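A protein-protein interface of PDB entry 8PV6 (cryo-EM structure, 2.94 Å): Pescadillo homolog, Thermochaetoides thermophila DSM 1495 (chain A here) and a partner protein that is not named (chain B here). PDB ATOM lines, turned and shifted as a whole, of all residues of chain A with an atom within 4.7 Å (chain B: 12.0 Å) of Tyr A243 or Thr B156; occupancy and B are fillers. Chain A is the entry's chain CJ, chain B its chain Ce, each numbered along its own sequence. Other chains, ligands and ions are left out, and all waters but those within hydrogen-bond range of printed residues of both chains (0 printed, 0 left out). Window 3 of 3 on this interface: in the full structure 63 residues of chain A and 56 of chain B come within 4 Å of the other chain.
O of Trp B160 lies within hydrogen-bond range of NH1 of Arg A244, at 3.2 Å.
O of Tyr A243 is in hydrogen-bond range of OG1 of Thr A247 (2.6 Å).
Tyr B157 touches Phe A240 (O to CE1, 3.3 Å).
Pro B159 touches Phe A240 (CD to CD1, 3.7 Å).
Trp B160 touches Phe A240 (CZ3 to O, 3.96 Å).
CG2 of Val A241 touches CH2 of Trp B160, at 3.97 Å.
OH of Tyr A243 touches CG2 of Thr B156 (3.4 Å).
O of Tyr B157 touches CD2 of Tyr A243, 3.9 Å away.
CE2 of Tyr A243 touches OD1 of Asp B158, at 3.3 Å.
Thr B156 touches one residue of chain A.
No residue of chain B comes within 4 Å of Gly A239.
No residue of chain B comes within 4 Å of Asn A242.
No residue of chain B comes within 4 Å of Leu A245.
No residue of chain B comes within 4 Å of Thr A247.
No residue of chain B comes within 4 Å of Tyr A253.
Of the printed residues of chain A, Tyr B157 touches Phe A240 (3.3 Å) and Tyr A243 (3.9 Å).
Of the printed residues of chain A, Trp B160 touches Phe A240 (3.96 Å), Val A241 (3.97 Å) and Arg A244 (3.2 Å).
Of the printed residues of chain B, Phe A240 touches Tyr B157, Pro B159 and Trp B160.
Of the printed residues of chain A, Pro B159 touches Phe A240.
The nearest residue of chain B that does not touch Tyr A243 is Pro B159 (5.7 Å).
The nearest printed residue of chain A that does not touch Thr B156 is Phe A240 (5.8 Å).
Of the 10 printed residues of chain A, 4 touch a printed residue of chain B.
Hydrophobic or aromatic side chains of chain B within 4 Å of the printed part of chain A: Tyr B157, Pro B159 and Trp B160.
Among the printed residues, no Asp or Glu carboxylate lies within 4 Å of a Lys or Arg side-chain nitrogen of the other chain.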
ATOM      1  N   GLY A 239      24.361  18.407 -16.632  1.00  0.00           N
ATOM      2  CA  GLY A 239      25.317  19.490 -16.827  1.00  0.00           C
ATOM      3  C   GLY A 239      25.518  20.328 -15.577  1.00  0.00           C
ATOM      4  O   GLY A 239      26.653  20.581 -15.158  1.00  0.00           O
ATOM      5  N   PHE A 240      24.418  20.724 -14.933  1.00  0.00           N
ATOM      6  CA  PHE A 240      24.512  21.516 -13.711  1.00  0.00           C
ATOM      7  C   PHE A 240      25.046  20.691 -12.548  1.00  0.00           C
ATOM      8  O   PHE A 240      25.782  21.215 -11.702  1.00  0.00           O
ATOM      9  CB  PHE A 240      23.151  22.111 -13.367  1.00  0.00           C
ATOM     10  CG  PHE A 240      22.692  23.155 -14.335  1.00  0.00           C
ATOM     11  CD1 PHE A 240      23.489  24.252 -14.610  1.00  0.00           C
ATOM     12  CD2 PHE A 240      21.469  23.040 -14.972  1.00  0.00           C
ATOM     13  CE1 PHE A 240      23.076  25.217 -15.502  1.00  0.00           C
ATOM     14  CE2 PHE A 240      21.051  24.002 -15.866  1.00  0.00           C
ATOM     15  CZ  PHE A 240      21.857  25.092 -16.130  1.00  0.00           C
ATOM     16  N   VAL A 241      24.687  19.404 -12.488  1.00  0.00           N
ATOM     17  CA  VAL A 241      25.215  18.539 -11.433  1.00  0.00           C
ATOM     18  C   VAL A 241      26.729  18.404 -11.557  1.00  0.00           C
ATOM     19  O   VAL A 241      27.461  18.527 -10.565  1.00  0.00           O
ATOM     20  CB  VAL A 241      24.515  17.167 -11.462  1.00  0.00           C
ATOM     21  CG1 VAL A 241      25.231  16.180 -10.563  1.00  0.00           C
ATOM     22  CG2 VAL A 241      23.071  17.305 -11.024  1.00  0.00           C
ATOM     23  N   ASN A 242      27.223  18.186 -12.781  1.00  0.00           N
ATOM     24  CA  ASN A 242      28.660  18.089 -13.016  1.00  0.00           C
ATOM     25  C   ASN A 242      29.368  19.397 -12.694  1.00  0.00           C
ATOM     26  O   ASN A 242      30.453  19.385 -12.101  1.00  0.00           O
ATOM     27  CB  ASN A 242      28.931  17.689 -14.465  1.00  0.00           C
ATOM     28  CG  ASN A 242      28.728  16.213 -14.710  1.00  0.00           C
ATOM     29  OD1 ASN A 242      28.544  15.437 -13.776  1.00  0.00           O
ATOM     30  ND2 ASN A 242      28.767  15.815 -15.975  1.00  0.00           N
ATOM     31  N   TYR A 243      28.771  20.531 -13.078  1.00  0.00           N
ATOM     32  CA  TYR A 243      29.383  21.823 -12.781  1.00  0.00           C
ATOM     33  C   TYR A 243      29.484  22.056 -11.278  1.00  0.00           C
ATOM     34  O   TYR A 243      30.523  22.507 -10.779  1.00  0.00           O
ATOM     35  CB  TYR A 243      28.593  22.951 -13.442  1.00  0.00           C
ATOM     36  CG  TYR A 243      29.004  24.329 -12.970  1.00  0.00           C
ATOM     37  CD1 TYR A 243      30.172  24.920 -13.433  1.00  0.00           C
ATOM     38  CD2 TYR A 243      28.219  25.043 -12.073  1.00  0.00           C
ATOM     39  CE1 TYR A 243      30.553  26.177 -13.007  1.00  0.00           C
ATOM     40  CE2 TYR A 243      28.595  26.299 -11.642  1.00  0.00           C
ATOM     41  CZ  TYR A 243      29.761  26.862 -12.114  1.00  0.00           C
ATOM     42  OH  TYR A 243      30.135  28.114 -11.688  1.00  0.00           O
ATOM     43  N   ARG A 244      28.415  21.742 -10.539  1.00  0.00           N
ATOM     44  CA  ARG A 244      28.433  21.957  -9.096  1.00  0.00           C
ATOM     45  C   ARG A 244      29.422  21.026  -8.407  1.00  0.00           C
ATOM     46  O   ARG A 244      30.119  21.436  -7.474  1.00  0.00           O
ATOM     47  CB  ARG A 244      27.034  21.784  -8.511  1.00  0.00           C
ATOM     48  CG  ARG A 244      26.975  22.035  -7.013  1.00  0.00           C
ATOM     49  CD  ARG A 244      25.554  22.054  -6.497  1.00  0.00           C
ATOM     50  NE  ARG A 244      25.505  22.046  -5.040  1.00  0.00           N
ATOM     51  CZ  ARG A 244      25.543  23.135  -4.285  1.00  0.00           C
ATOM     52  NH1 ARG A 244      25.634  24.342  -4.817  1.00  0.00           N
ATOM     53  NH2 ARG A 244      25.488  23.008  -2.962  1.00  0.00           N
ATOM     54  N   LEU A 245      29.511  19.771  -8.860  1.00  0.00           N
ATOM     55  CA  LEU A 245      30.462  18.840  -8.255  1.00  0.00           C
ATOM     56  C   LEU A 245      31.907  19.248  -8.537  1.00  0.00           C
ATOM     57  O   LEU A 245      32.762  19.179  -7.641  1.00  0.00           O
ATOM     58  CB  LEU A 245      30.185  17.421  -8.748  1.00  0.00           C
ATOM     59  CG  LEU A 245      28.904  16.787  -8.197  1.00  0.00           C
ATOM     60  CD1 LEU A 245      28.636  15.435  -8.835  1.00  0.00           C
ATOM     61  CD2 LEU A 245      28.975  16.662  -6.685  1.00  0.00           C
ATOM     62  N   TYR A 246      32.193  19.689  -9.767  1.00  0.00           N
ATOM     63  CA  TYR A 246      33.535  20.161 -10.097  1.00  0.00           C
ATOM     64  C   TYR A 246      33.898  21.411  -9.304  1.00  0.00           C
ATOM     65  O   TYR A 246      35.035  21.546  -8.837  1.00  0.00           O
ATOM     66  CB  TYR A 246      33.646  20.434 -11.596  1.00  0.00           C
ATOM     67  CG  TYR A 246      34.063  19.241 -12.425  1.00  0.00           C
ATOM     68  CD1 TYR A 246      33.301  18.080 -12.444  1.00  0.00           C
ATOM     69  CD2 TYR A 246      35.217  19.277 -13.195  1.00  0.00           C
ATOM     70  CE1 TYR A 246      33.676  16.992 -13.205  1.00  0.00           C
ATOM     71  CE2 TYR A 246      35.601  18.193 -13.956  1.00  0.00           C
ATOM     72  CZ  TYR A 246      34.826  17.054 -13.957  1.00  0.00           C
ATOM     73  OH  TYR A 246      35.202  15.970 -14.713  1.00  0.00           O
ATOM     74  N   THR A 247      32.947  22.336  -9.139  1.00  0.00           N
ATOM     75  CA  THR A 247      33.206  23.521  -8.330  1.00  0.00           C
ATOM     76  C   THR A 247      33.393  23.167  -6.858  1.00  0.00           C
ATOM     77  O   THR A 247      34.212  23.790  -6.173  1.00  0.00           O
ATOM     78  CB  THR A 247      32.065  24.526  -8.497  1.00  0.00           C
ATOM     79  OG1 THR A 247      31.754  24.662  -9.889  1.00  0.00           O
ATOM     80  CG2 THR A 247      32.460  25.887  -7.948  1.00  0.00           C
ATOM     81  N   TYR A 253      35.311  23.688 -14.758  1.00  0.00           N
ATOM     82  CA  TYR A 253      34.296  23.059 -15.587  1.00  0.00           C
ATOM     83  C   TYR A 253      33.894  24.039 -16.682  1.00  0.00           C
ATOM     84  O   TYR A 253      33.689  25.232 -16.396  1.00  0.00           O
ATOM     85  CB  TYR A 253      33.072  22.642 -14.762  1.00  0.00           C
ATOM     86  CG  TYR A 253      32.084  21.801 -15.537  1.00  0.00           C
ATOM     87  CD1 TYR A 253      32.263  20.430 -15.665  1.00  0.00           C
ATOM     88  CD2 TYR A 253      30.979  22.378 -16.148  1.00  0.00           C
ATOM     89  CE1 TYR A 253      31.366  19.657 -16.375  1.00  0.00           C
ATOM     90  CE2 TYR A 253      30.078  21.612 -16.860  1.00  0.00           C
ATOM     91  CZ  TYR A 253      30.277  20.253 -16.971  1.00  0.00           C
ATOM     92  OH  TYR A 253      29.381  19.489 -17.679  1.00  0.00           O
ATOM     93  N   THR B 156      28.363  31.250 -17.000  1.00  0.00           N
ATOM     94  CA  THR B 156      27.776  29.990 -16.559  1.00  0.00           C
ATOM     95  C   THR B 156      26.574  30.231 -15.653  1.00  0.00           C
ATOM     96  O   THR B 156      26.163  31.372 -15.443  1.00  0.00           O
ATOM     97  CB  THR B 156      28.805  29.115 -15.820  1.00  0.00           C
ATOM     98  OG1 THR B 156      28.215  27.852 -15.492  1.00  0.00           O
ATOM     99  CG2 THR B 156      29.280  29.803 -14.546  1.00  0.00           C
ATOM    100  N   TYR B 157      26.012  29.151 -15.118  1.00  0.00           N
ATOM    101  CA  TYR B 157      24.828  29.246 -14.275  1.00  0.00           C
ATOM    102  C   TYR B 157      24.903  28.163 -13.212  1.00  0.00           C
ATOM    103  O   TYR B 157      25.116  26.987 -13.522  1.00  0.00           O
ATOM    104  CB  TYR B 157      23.548  29.109 -15.108  1.00  0.00           C
ATOM    105  CG  TYR B 157      22.267  29.235 -14.318  1.00  0.00           C
ATOM    106  CD1 TYR B 157      21.815  30.475 -13.886  1.00  0.00           C
ATOM    107  CD2 TYR B 157      21.497  28.118 -14.028  1.00  0.00           C
ATOM    108  CE1 TYR B 157      20.638  30.595 -13.169  1.00  0.00           C
ATOM    109  CE2 TYR B 157      20.320  28.228 -13.314  1.00  0.00           C
ATOM    110  CZ  TYR B 157      19.896  29.468 -12.888  1.00  0.00           C
ATOM    111  OH  TYR B 157      18.723  29.578 -12.176  1.00  0.00           O
ATOM    112  N   ASP B 158      24.729  28.574 -11.957  1.00  0.00           N
ATOM    113  CA  ASP B 158      24.857  27.682 -10.805  1.00  0.00           C
ATOM    114  C   ASP B 158      23.563  27.661 -10.006  1.00  0.00           C
ATOM    115  O   ASP B 158      23.315  28.548  -9.179  1.00  0.00           O
ATOM    116  CB  ASP B 158      26.024  28.098  -9.912  1.00  0.00           C
ATOM    117  CG  ASP B 158      26.406  27.021  -8.917  1.00  0.00           C
ATOM    118  OD1 ASP B 158      26.390  25.830  -9.294  1.00  0.00           O
ATOM    119  OD2 ASP B 158      26.723  27.362  -7.759  1.00  0.00           O
ATOM    120  N   PRO B 159      22.711  26.660 -10.222  1.00  0.00           N
ATOM    121  CA  PRO B 159      21.565  26.466  -9.327  1.00  0.00           C
ATOM    122  C   PRO B 159      22.000  25.936  -7.968  1.00  0.00           C
ATOM    123  O   PRO B 159      23.176  25.615  -7.768  1.00  0.00           O
ATOM    124  CB  PRO B 159      20.698  25.450 -10.084  1.00  0.00           C
ATOM    125  CG  PRO B 159      21.659  24.737 -10.968  1.00  0.00           C
ATOM    126  CD  PRO B 159      22.629  25.789 -11.405  1.00  0.00           C
ATOM    127  N   TRP B 160      21.058  25.857  -7.031  1.00  0.00           N
ATOM    128  CA  TRP B 160      21.205  25.381  -5.659  1.00  0.00           C
ATOM    129  C   TRP B 160      22.203  26.225  -4.875  1.00  0.00           C
ATOM    130  O   TRP B 160      22.858  25.695  -3.969  1.00  0.00           O
ATOM    131  CB  TRP B 160      21.614  23.899  -5.580  1.00  0.00           C
ATOM    132  CG  TRP B 160      20.793  23.012  -6.463  1.00  0.00           C
ATOM    133  CD1 TRP B 160      19.469  22.722  -6.327  1.00  0.00           C
ATOM    134  CD2 TRP B 160      21.237  22.319  -7.634  1.00  0.00           C
ATOM    135  NE1 TRP B 160      19.063  21.878  -7.331  1.00  0.00           N
ATOM    136  CE2 TRP B 160      20.131  21.618  -8.148  1.00  0.00           C
ATOM    137  CE3 TRP B 160      22.464  22.217  -8.294  1.00  0.00           C
ATOM    138  CZ2 TRP B 160      20.214  20.827  -9.290  1.00  0.00           C
ATOM    139  CZ3 TRP B 160      22.546  21.434  -9.426  1.00  0.00           C
ATOM    140  CH2 TRP B 160      21.428  20.749  -9.914  1.00  0.00           C
ATOM    141  N   ALA B 161      22.340  27.510  -5.183  1.00  0.00           N
ATOM    142  CA  ALA B 161      23.256  28.382  -4.461  1.00  0.00           C
ATOM    143  C   ALA B 161      22.730  29.812  -4.434  1.00  0.00           C
ATOM    144  O   ALA B 161      21.957  30.215  -5.301  1.00  0.00           O
ATOM    145  CB  ALA B 161      24.638  28.335  -5.088  1.00  0.00           C
